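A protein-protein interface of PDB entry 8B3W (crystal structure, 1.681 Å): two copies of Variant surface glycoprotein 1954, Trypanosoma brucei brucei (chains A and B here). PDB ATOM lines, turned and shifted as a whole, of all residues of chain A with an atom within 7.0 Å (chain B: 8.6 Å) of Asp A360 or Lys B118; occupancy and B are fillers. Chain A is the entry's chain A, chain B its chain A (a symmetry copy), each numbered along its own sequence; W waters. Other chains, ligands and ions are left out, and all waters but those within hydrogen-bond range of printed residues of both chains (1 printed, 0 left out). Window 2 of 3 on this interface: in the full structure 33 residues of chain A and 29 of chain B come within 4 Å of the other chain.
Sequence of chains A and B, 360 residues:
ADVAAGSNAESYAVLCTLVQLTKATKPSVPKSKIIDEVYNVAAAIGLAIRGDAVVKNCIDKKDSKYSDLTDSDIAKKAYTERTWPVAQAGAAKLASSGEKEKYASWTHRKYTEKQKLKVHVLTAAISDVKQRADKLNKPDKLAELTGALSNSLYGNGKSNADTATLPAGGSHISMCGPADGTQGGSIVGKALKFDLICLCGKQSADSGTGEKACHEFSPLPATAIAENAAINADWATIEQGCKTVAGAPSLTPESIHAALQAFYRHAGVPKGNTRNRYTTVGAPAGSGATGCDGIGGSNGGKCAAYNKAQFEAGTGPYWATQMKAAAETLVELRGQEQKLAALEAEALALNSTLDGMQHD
O of Asp A360 sits at hydrogen-bond distance from NZ of Lys B118 (2.7 Å).
The side-chain carboxylate of Asp A355 lies within hydrogen-bond range of the side-chain amide nitrogen of Gln A358 (2.8 Å).
Among the printed residues, merely in contact across the chains: Ser A352 with Ala B125 (3.3 Å), Gly A356 with Lys B118 (3.3 Å), His A359 with Leu B117 (3.5 Å), Ser A352 with Val B121 (3.5 Å), Asp A355 with Val B121 (3.7 Å), Gly A356 with Val B121 (3.9 Å) and His A359 with Lys B118 (3.9 Å).
Tyr A111 touches none of the printed residues of chain B. Of the printed residues of chain B, Ser A352 touches Val B121 (3.5 Å) and Ala B125 (3.3 Å). Of the printed residues of chain B, His A359 touches Leu B117 and Lys B118. Of the printed residues of chain B, Asp A360 touches Lys B118. Lys B118 touches just these residues of chain A: Gly A356 (3.3 Å), His A359 (3.9 Å) and Asp A360 (2.7 Å). Met B357 touches none of the printed residues of chain A. The nearest residue of chain A that does not touch Lys B118 is Met A357 (4.4 Å). The nearest printed residue of chain B that does not touch Ser A352 is Leu B122 (4.3 Å).
Of the 11 printed residues of chain A, 5 touch a printed residue of chain B. Printed residues of chain A that touch a printed residue of chain B: Ser A352, Asp A355, Gly A356, His A359 and Asp A360. Hydrophobic or aromatic side chains of chain A that line the printed part of chain B: His A359. Printed residues of chain B that touch a printed residue of chain A: Leu B117, Lys B118, Val B121 and Ala B125. Among the printed residues, no Asp or Glu carboxylate lies within 4 Å of a Lys or Arg side-chain nitrogen of the other chain.
Asp A360 touches Lys B118, but with the chains exchanged Lys A118 does not touch Asp B360 (7.8 Å). Positions printed for both chains: 115, 118, 353, 357 and 360. Of the 8 pairs that touch across the chains among the printed residues, none has its exchanged pair printed and touching as well.
Water W1 bridges the side-chain hydroxyl of Thr B353 and the side-chain hydroxyl of Thr A353.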
ATOM      1  N   TYR A 111      12.212 -16.653  -2.401  1.00  0.00           N
ATOM      2  CA  TYR A 111      10.814 -17.045  -2.550  1.00  0.00           C
ATOM      3  C   TYR A 111      10.503 -18.252  -1.670  1.00  0.00           C
ATOM      4  O   TYR A 111      11.374 -19.084  -1.398  1.00  0.00           O
ATOM      5  CB  TYR A 111      10.477 -17.372  -4.036  1.00  0.00           C
ATOM      6  CG  TYR A 111      10.742 -16.226  -4.997  1.00  0.00           C
ATOM      7  CD1 TYR A 111       9.787 -15.242  -5.216  1.00  0.00           C
ATOM      8  CD2 TYR A 111      11.951 -16.122  -5.674  1.00  0.00           C
ATOM      9  CE1 TYR A 111      10.029 -14.186  -6.087  1.00  0.00           C
ATOM     10  CE2 TYR A 111      12.200 -15.069  -6.548  1.00  0.00           C
ATOM     11  CZ  TYR A 111      11.233 -14.107  -6.746  1.00  0.00           C
ATOM     12  OH  TYR A 111      11.473 -13.057  -7.603  1.00  0.00           O
ATOM     13  N   GLN A 115       5.568 -20.161  -3.309  1.00  0.00           N
ATOM     14  CA  GLN A 115       5.807 -19.235  -4.413  1.00  0.00           C
ATOM     15  C   GLN A 115       6.540 -19.934  -5.547  1.00  0.00           C
ATOM     16  O   GLN A 115       6.169 -19.801  -6.717  1.00  0.00           O
ATOM     17  CB  GLN A 115       6.599 -18.021  -3.930  1.00  0.00           C
ATOM     18  CG  GLN A 115       5.787 -17.037  -3.101  1.00  0.00           C
ATOM     19  CD  GLN A 115       6.560 -15.767  -2.775  1.00  0.00           C
ATOM     20  OE1 GLN A 115       7.722 -15.824  -2.362  1.00  0.00           O
ATOM     21  NE2 GLN A 115       5.921 -14.611  -2.971  1.00  0.00           N
ATOM     22  N   LYS A 118       4.105 -22.211  -7.407  1.00  0.00           N
ATOM     23  CA  LYS A 118       3.198 -21.501  -8.299  1.00  0.00           C
ATOM     24  C   LYS A 118       3.941 -20.964  -9.517  1.00  0.00           C
ATOM     25  O   LYS A 118       3.417 -20.983 -10.635  1.00  0.00           O
ATOM     26  CB  LYS A 118       2.496 -20.371  -7.547  1.00  0.00           C
ATOM     27  CG  LYS A 118       1.215 -19.941  -8.211  1.00  0.00           C
ATOM     28  CD  LYS A 118       0.789 -18.536  -7.803  1.00  0.00           C
ATOM     29  CE  LYS A 118      -0.072 -18.524  -6.550  1.00  0.00           C
ATOM     30  NZ  LYS A 118      -0.752 -17.199  -6.389  1.00  0.00           N
ATOM     31  N   SER A 352       2.749 -12.541 -18.878  1.00  0.00           N
ATOM     32  CA  SER A 352       2.427 -11.331 -18.127  1.00  0.00           C
ATOM     33  C   SER A 352       2.139 -11.660 -16.674  1.00  0.00           C
ATOM     34  O   SER A 352       2.621 -10.977 -15.766  1.00  0.00           O
ATOM     35  CB  SER A 352       1.231 -10.618 -18.767  1.00  0.00           C
ATOM     36  OG  SER A 352       1.625 -10.090 -20.019  1.00  0.00           O
ATOM     37  N   THR A 353       1.353 -12.712 -16.443  1.00  0.00           N
ATOM     38  CA  THR A 353       1.066 -13.150 -15.085  1.00  0.00           C
ATOM     39  C   THR A 353       2.342 -13.512 -14.351  1.00  0.00           C
ATOM     40  O   THR A 353       2.526 -13.144 -13.185  1.00  0.00           O
ATOM     41  CB  THR A 353       0.112 -14.343 -15.136  1.00  0.00           C
ATOM     42  OG1 THR A 353      -1.067 -13.958 -15.834  1.00  0.00           O
ATOM     43  CG2 THR A 353      -0.278 -14.760 -13.772  1.00  0.00           C
ATOM     44  N   ASP A 355       5.348 -12.392 -15.054  1.00  0.00           N
ATOM     45  CA  ASP A 355       6.083 -11.145 -14.848  1.00  0.00           C
ATOM     46  C   ASP A 355       5.673 -10.496 -13.537  1.00  0.00           C
ATOM     47  O   ASP A 355       6.520 -10.085 -12.737  1.00  0.00           O
ATOM     48  CB  ASP A 355       5.826 -10.197 -16.019  1.00  0.00           C
ATOM     49  CG  ASP A 355       6.684  -8.958 -15.977  1.00  0.00           C
ATOM     50  OD1 ASP A 355       7.633  -8.902 -15.173  1.00  0.00           O
ATOM     51  OD2 ASP A 355       6.424  -8.050 -16.784  1.00  0.00           O
ATOM     52  N   GLY A 356       4.362 -10.418 -13.290  1.00  0.00           N
ATOM     53  CA  GLY A 356       3.884  -9.769 -12.088  1.00  0.00           C
ATOM     54  C   GLY A 356       4.282 -10.483 -10.815  1.00  0.00           C
ATOM     55  O   GLY A 356       4.416  -9.852  -9.763  1.00  0.00           O
ATOM     56  N   MET A 357       4.478 -11.803 -10.882  1.00  0.00           N
ATOM     57  CA  MET A 357       4.835 -12.557  -9.688  1.00  0.00           C
ATOM     58  C   MET A 357       6.239 -12.244  -9.177  1.00  0.00           C
ATOM     59  O   MET A 357       6.552 -12.593  -8.035  1.00  0.00           O
ATOM     60  CB  MET A 357       4.708 -14.055  -9.960  1.00  0.00           C
ATOM     61  CG  MET A 357       3.264 -14.525 -10.028  1.00  0.00           C
ATOM     62  SD  MET A 357       3.100 -16.202 -10.685  1.00  0.00           S
ATOM     63  CE  MET A 357       3.767 -17.092  -9.290  1.00  0.00           C
ATOM     64  N   GLN A 358       7.097 -11.599  -9.976  1.00  0.00           N
ATOM     65  CA  GLN A 358       8.432 -11.285  -9.468  1.00  0.00           C
ATOM     66  C   GLN A 358       8.347 -10.469  -8.187  1.00  0.00           C
ATOM     67  O   GLN A 358       9.328 -10.391  -7.437  1.00  0.00           O
ATOM     68  CB  GLN A 358       9.260 -10.541 -10.523  1.00  0.00           C
ATOM     69  CG  GLN A 358       8.922  -9.053 -10.699  1.00  0.00           C
ATOM     70  CD  GLN A 358       9.767  -8.388 -11.794  1.00  0.00           C
ATOM     71  OE1 GLN A 358      10.752  -7.713 -11.511  1.00  0.00           O
ATOM     72  NE2 GLN A 358       9.378  -8.582 -13.046  1.00  0.00           N
ATOM     73  N   HIS A 359       7.185  -9.881  -7.915  1.00  0.00           N
ATOM     74  CA  HIS A 359       6.935  -9.143  -6.684  1.00  0.00           C
ATOM     75  C   HIS A 359       6.478 -10.080  -5.566  1.00  0.00           C
ATOM     76  O   HIS A 359       7.114 -10.148  -4.507  1.00  0.00           O
ATOM     77  CB  HIS A 359       5.908  -8.042  -6.973  1.00  0.00           C
ATOM     78  CG  HIS A 359       6.298  -7.157  -8.120  1.00  0.00           C
ATOM     79  ND1 HIS A 359       7.546  -6.578  -8.219  1.00  0.00           N
ATOM     80  CD2 HIS A 359       5.615  -6.765  -9.223  1.00  0.00           C
ATOM     81  CE1 HIS A 359       7.612  -5.861  -9.326  1.00  0.00           C
ATOM     82  NE2 HIS A 359       6.454  -5.957  -9.953  1.00  0.00           N
ATOM     83  N   ASP A 360       5.388 -10.814  -5.789  1.00  0.00           N
ATOM     84  CA  ASP A 360       4.965 -11.856  -4.852  1.00  0.00           C
ATOM     85  C   ASP A 360       3.773 -12.639  -5.392  1.00  0.00           C
ATOM     86  O   ASP A 360       2.843 -12.067  -5.952  1.00  0.00           O
ATOM     87  CB  ASP A 360       4.614 -11.256  -3.486  1.00  0.00           C
ATOM     88  N   ILE B  49      -5.860   3.221  -9.188  1.00  0.00           N
ATOM     89  CA  ILE B  49      -5.000   2.848  -8.068  1.00  0.00           C
ATOM     90  C   ILE B  49      -3.862   3.830  -7.857  1.00  0.00           C
ATOM     91  O   ILE B  49      -3.088   3.670  -6.908  1.00  0.00           O
ATOM     92  CB  ILE B  49      -4.379   1.441  -8.210  1.00  0.00           C
ATOM     93  CG1 ILE B  49      -3.460   1.353  -9.431  1.00  0.00           C
ATOM     94  CG2 ILE B  49      -5.466   0.366  -8.271  1.00  0.00           C
ATOM     95  CD1 ILE B  49      -2.539   0.143  -9.388  1.00  0.00           C
ATOM     96  N   TRP B 106     -11.620  -0.577  -6.689  1.00  0.00           N
ATOM     97  CA  TRP B 106     -10.271  -0.054  -7.027  1.00  0.00           C
ATOM     98  C   TRP B 106     -10.034   1.348  -6.465  1.00  0.00           C
ATOM     99  O   TRP B 106      -8.886   1.632  -6.139  1.00  0.00           O
ATOM    100  CB  TRP B 106     -10.061  -0.079  -8.543  1.00  0.00           C
ATOM    101  CG  TRP B 106     -10.021  -1.476  -9.064  1.00  0.00           C
ATOM    102  CD1 TRP B 106     -11.030  -2.139  -9.687  1.00  0.00           C
ATOM    103  CD2 TRP B 106      -8.938  -2.414  -8.941  1.00  0.00           C
ATOM    104  NE1 TRP B 106     -10.624  -3.406  -9.993  1.00  0.00           N
ATOM    105  CE2 TRP B 106      -9.355  -3.605  -9.553  1.00  0.00           C
ATOM    106  CE3 TRP B 106      -7.656  -2.363  -8.398  1.00  0.00           C
ATOM    107  CZ2 TRP B 106      -8.543  -4.728  -9.653  1.00  0.00           C
ATOM    108  CZ3 TRP B 106      -6.851  -3.475  -8.483  1.00  0.00           C
ATOM    109  CH2 TRP B 106      -7.291  -4.644  -9.099  1.00  0.00           C
ATOM    110  N   THR B 112      -0.717  -2.034  -1.587  1.00  0.00           N
ATOM    111  CA  THR B 112       0.726  -1.901  -1.408  1.00  0.00           C
ATOM    112  C   THR B 112       1.392  -1.375  -2.677  1.00  0.00           C
ATOM    113  O   THR B 112       0.841  -1.452  -3.774  1.00  0.00           O
ATOM    114  CB  THR B 112       1.343  -3.251  -1.059  1.00  0.00           C
ATOM    115  OG1 THR B 112       0.577  -3.869  -0.019  1.00  0.00           O
ATOM    116  CG2 THR B 112       2.778  -3.084  -0.578  1.00  0.00           C
ATOM    117  N   GLU B 113       2.614  -0.847  -2.517  1.00  0.00           N
ATOM    118  CA  GLU B 113       3.413  -0.498  -3.686  1.00  0.00           C
ATOM    119  C   GLU B 113       3.591  -1.705  -4.591  1.00  0.00           C
ATOM    120  O   GLU B 113       3.547  -1.581  -5.819  1.00  0.00           O
ATOM    121  CB  GLU B 113       4.780   0.042  -3.272  1.00  0.00           C
ATOM    122  CG  GLU B 113       4.725   1.273  -2.391  1.00  0.00           C
ATOM    123  CD  GLU B 113       3.805   2.352  -2.941  1.00  0.00           C
ATOM    124  OE1 GLU B 113       3.918   2.686  -4.140  1.00  0.00           O
ATOM    125  OE2 GLU B 113       2.954   2.854  -2.180  1.00  0.00           O
ATOM    126  N   LYS B 114       3.789  -2.884  -3.993  1.00  0.00           N
ATOM    127  CA  LYS B 114       3.954  -4.109  -4.768  1.00  0.00           C
ATOM    128  C   LYS B 114       2.663  -4.483  -5.482  1.00  0.00           C
ATOM    129  O   LYS B 114       2.673  -4.773  -6.683  1.00  0.00           O
ATOM    130  CB  LYS B 114       4.411  -5.251  -3.855  1.00  0.00           C
ATOM    131  N   GLN B 115       1.541  -4.491  -4.754  1.00  0.00           N
ATOM    132  CA  GLN B 115       0.250  -4.755  -5.384  1.00  0.00           C
ATOM    133  C   GLN B 115       0.027  -3.821  -6.562  1.00  0.00           C
ATOM    134  O   GLN B 115      -0.384  -4.252  -7.643  1.00  0.00           O
ATOM    135  CB  GLN B 115      -0.881  -4.612  -4.366  1.00  0.00           C
ATOM    136  CG  GLN B 115      -0.976  -5.761  -3.373  1.00  0.00           C
ATOM    137  CD  GLN B 115      -2.206  -5.667  -2.482  1.00  0.00           C
ATOM    138  OE1 GLN B 115      -2.509  -4.601  -1.938  1.00  0.00           O
ATOM    139  NE2 GLN B 115      -2.925  -6.782  -2.335  1.00  0.00           N
ATOM    140  N   LYS B 116       0.337  -2.541  -6.386  1.00  0.00           N
ATOM    141  CA  LYS B 116       0.175  -1.593  -7.479  1.00  0.00           C
ATOM    142  C   LYS B 116       1.113  -1.912  -8.637  1.00  0.00           C
ATOM    143  O   LYS B 116       0.718  -1.801  -9.803  1.00  0.00           O
ATOM    144  CB  LYS B 116       0.397  -0.181  -6.956  1.00  0.00           C
ATOM    145  CG  LYS B 116      -0.698   0.245  -5.970  1.00  0.00           C
ATOM    146  CD  LYS B 116      -0.582   1.705  -5.563  1.00  0.00           C
ATOM    147  CE  LYS B 116       0.571   1.955  -4.621  1.00  0.00           C
ATOM    148  NZ  LYS B 116       0.729   3.423  -4.345  1.00  0.00           N
ATOM    149  N   LEU B 117       2.350  -2.317  -8.340  1.00  0.00           N
ATOM    150  CA  LEU B 117       3.255  -2.776  -9.393  1.00  0.00           C
ATOM    151  C   LEU B 117       2.631  -3.910 -10.189  1.00  0.00           C
ATOM    152  O   LEU B 117       2.549  -3.849 -11.421  1.00  0.00           O
ATOM    153  CB  LEU B 117       4.581  -3.243  -8.794  1.00  0.00           C
ATOM    154  CG  LEU B 117       5.502  -2.156  -8.260  1.00  0.00           C
ATOM    155  CD1 LEU B 117       6.651  -2.812  -7.519  1.00  0.00           C
ATOM    156  CD2 LEU B 117       5.996  -1.232  -9.386  1.00  0.00           C
ATOM    157  N   LYS B 118       2.186  -4.962  -9.497  1.00  0.00           N
ATOM    158  CA  LYS B 118       1.662  -6.127 -10.197  1.00  0.00           C
ATOM    159  C   LYS B 118       0.412  -5.768 -10.994  1.00  0.00           C
ATOM    160  O   LYS B 118       0.213  -6.261 -12.108  1.00  0.00           O
ATOM    161  CB  LYS B 118       1.372  -7.251  -9.203  1.00  0.00           C
ATOM    162  CG  LYS B 118       1.329  -8.606  -9.858  1.00  0.00           C
ATOM    163  CD  LYS B 118       0.557  -9.630  -9.033  1.00  0.00           C
ATOM    164  CE  LYS B 118       1.433 -10.348  -8.020  1.00  0.00           C
ATOM    165  NZ  LYS B 118       0.738 -11.566  -7.492  1.00  0.00           N
ATOM    166  N   VAL B 119      -0.432  -4.894 -10.453  1.00  0.00           N
ATOM    167  CA  VAL B 119      -1.600  -4.474 -11.210  1.00  0.00           C
ATOM    168  C   VAL B 119      -1.167  -3.803 -12.508  1.00  0.00           C
ATOM    169  O   VAL B 119      -1.732  -4.067 -13.577  1.00  0.00           O
ATOM    170  CB  VAL B 119      -2.483  -3.561 -10.346  1.00  0.00           C
ATOM    171  CG1 VAL B 119      -3.493  -2.824 -11.202  1.00  0.00           C
ATOM    172  CG2 VAL B 119      -3.196  -4.385  -9.327  1.00  0.00           C
ATOM    173  N   HIS B 120      -0.125  -2.968 -12.452  1.00  0.00           N
ATOM    174  CA  HIS B 120       0.261  -2.223 -13.644  1.00  0.00           C
ATOM    175  C   HIS B 120       0.945  -3.111 -14.670  1.00  0.00           C
ATOM    176  O   HIS B 120       0.919  -2.791 -15.864  1.00  0.00           O
ATOM    177  CB  HIS B 120       1.156  -1.047 -13.271  1.00  0.00           C
ATOM    178  CG  HIS B 120       0.400   0.118 -12.711  1.00  0.00           C
ATOM    179  ND1 HIS B 120       0.882   0.888 -11.678  1.00  0.00           N
ATOM    180  CD2 HIS B 120      -0.800   0.648 -13.048  1.00  0.00           C
ATOM    181  CE1 HIS B 120       0.016   1.848 -11.407  1.00  0.00           C
ATOM    182  NE2 HIS B 120      -1.017   1.723 -12.222  1.00  0.00           N
ATOM    183  N   VAL B 121       1.553  -4.217 -14.248  1.00  0.00           N
ATOM    184  CA  VAL B 121       2.032  -5.200 -15.222  1.00  0.00           C
ATOM    185  C   VAL B 121       0.877  -5.672 -16.099  1.00  0.00           C
ATOM    186  O   VAL B 121       0.996  -5.744 -17.329  1.00  0.00           O
ATOM    187  CB  VAL B 121       2.710  -6.383 -14.502  1.00  0.00           C
ATOM    188  CG1 VAL B 121       3.034  -7.510 -15.483  1.00  0.00           C
ATOM    189  CG2 VAL B 121       3.943  -5.914 -13.811  1.00  0.00           C
ATOM    190  N   LEU B 122      -0.267  -5.965 -15.478  1.00  0.00           N
ATOM    191  CA  LEU B 122      -1.427  -6.461 -16.208  1.00  0.00           C
ATOM    192  C   LEU B 122      -2.065  -5.368 -17.058  1.00  0.00           C
ATOM    193  O   LEU B 122      -2.419  -5.611 -18.223  1.00  0.00           O
ATOM    194  CB  LEU B 122      -2.446  -7.041 -15.227  1.00  0.00           C
ATOM    195  CG  LEU B 122      -2.045  -8.343 -14.519  1.00  0.00           C
ATOM    196  CD1 LEU B 122      -3.261  -9.019 -13.879  1.00  0.00           C
ATOM    197  CD2 LEU B 122      -1.354  -9.317 -15.474  1.00  0.00           C
ATOM    198  N   THR B 123      -2.184  -4.150 -16.520  1.00  0.00           N
ATOM    199  CA  THR B 123      -2.774  -3.076 -17.314  1.00  0.00           C
ATOM    200  C   THR B 123      -1.878  -2.708 -18.489  1.00  0.00           C
ATOM    201  O   THR B 123      -2.377  -2.482 -19.601  1.00  0.00           O
ATOM    202  CB  THR B 123      -3.087  -1.859 -16.441  1.00  0.00           C
ATOM    203  OG1 THR B 123      -1.893  -1.317 -15.877  1.00  0.00           O
ATOM    204  CG2 THR B 123      -4.026  -2.272 -15.333  1.00  0.00           C
ATOM    205  N   ALA B 124      -0.557  -2.706 -18.287  1.00  0.00           N
ATOM    206  CA  ALA B 124       0.351  -2.460 -19.409  1.00  0.00           C
ATOM    207  C   ALA B 124       0.252  -3.570 -20.449  1.00  0.00           C
ATOM    208  O   ALA B 124       0.346  -3.313 -21.657  1.00  0.00           O
ATOM    209  CB  ALA B 124       1.796  -2.335 -18.914  1.00  0.00           C
ATOM    210  N   ALA B 125       0.089  -4.818 -19.996  1.00  0.00           N
ATOM    211  CA  ALA B 125      -0.057  -5.927 -20.930  1.00  0.00           C
ATOM    212  C   ALA B 125      -1.335  -5.784 -21.743  1.00  0.00           C
ATOM    213  O   ALA B 125      -1.339  -6.068 -22.942  1.00  0.00           O
ATOM    214  CB  ALA B 125      -0.025  -7.267 -20.183  1.00  0.00           C
ATOM    215  N   THR B 353      -7.828 -12.183 -14.696  1.00  0.00           N
ATOM    216  CA  THR B 353      -6.805 -12.181 -13.661  1.00  0.00           C
ATOM    217  C   THR B 353      -6.787 -10.860 -12.918  1.00  0.00           C
ATOM    218  O   THR B 353      -6.695 -10.829 -11.685  1.00  0.00           O
ATOM    219  CB  THR B 353      -5.446 -12.463 -14.301  1.00  0.00           C
ATOM    220  OG1 THR B 353      -5.510 -13.708 -14.987  1.00  0.00           O
ATOM    221  CG2 THR B 353      -4.390 -12.560 -13.271  1.00  0.00           C
ATOM    222  N   LEU B 354      -6.870  -9.750 -13.657  1.00  0.00           N
ATOM    223  CA  LEU B 354      -6.906  -8.431 -13.030  1.00  0.00           C
ATOM    224  C   LEU B 354      -8.160  -8.264 -12.177  1.00  0.00           C
ATOM    225  O   LEU B 354      -8.102  -7.705 -11.071  1.00  0.00           O
ATOM    226  CB  LEU B 354      -6.829  -7.344 -14.112  1.00  0.00           C
ATOM    227  CG  LEU B 354      -6.797  -5.853 -13.761  1.00  0.00           C
ATOM    228  CD1 LEU B 354      -5.639  -5.456 -12.828  1.00  0.00           C
ATOM    229  CD2 LEU B 354      -6.719  -5.040 -15.035  1.00  0.00           C
ATOM    230  N   MET B 357      -7.710  -9.658  -8.769  1.00  0.00           N
ATOM    231  CA  MET B 357      -6.786  -8.946  -7.897  1.00  0.00           C
ATOM    232  C   MET B 357      -7.455  -7.838  -7.089  1.00  0.00           C
ATOM    233  O   MET B 357      -6.856  -7.356  -6.122  1.00  0.00           O
ATOM    234  CB  MET B 357      -5.639  -8.361  -8.720  1.00  0.00           C
ATOM    235  CG  MET B 357      -4.649  -9.416  -9.188  1.00  0.00           C
ATOM    236  SD  MET B 357      -3.497  -8.794 -10.436  1.00  0.00           S
ATOM    237  CE  MET B 357      -2.520  -7.737  -9.382  1.00  0.00           C
ATOM    238  N   ASP B 360      -6.862  -9.139  -3.596  1.00  0.00           N
ATOM    239  CA  ASP B 360      -5.463  -8.989  -3.191  1.00  0.00           C
ATOM    240  C   ASP B 360      -4.524  -9.690  -4.167  1.00  0.00           C
ATOM    241  O   ASP B 360      -4.794 -10.799  -4.617  1.00  0.00           O
ATOM    242  CB  ASP B 360      -5.239  -9.532  -1.776  1.00  0.00           C
HETATM  243  O   HOH W   1      -3.443 -15.210 -15.809  1.00  0.00           O
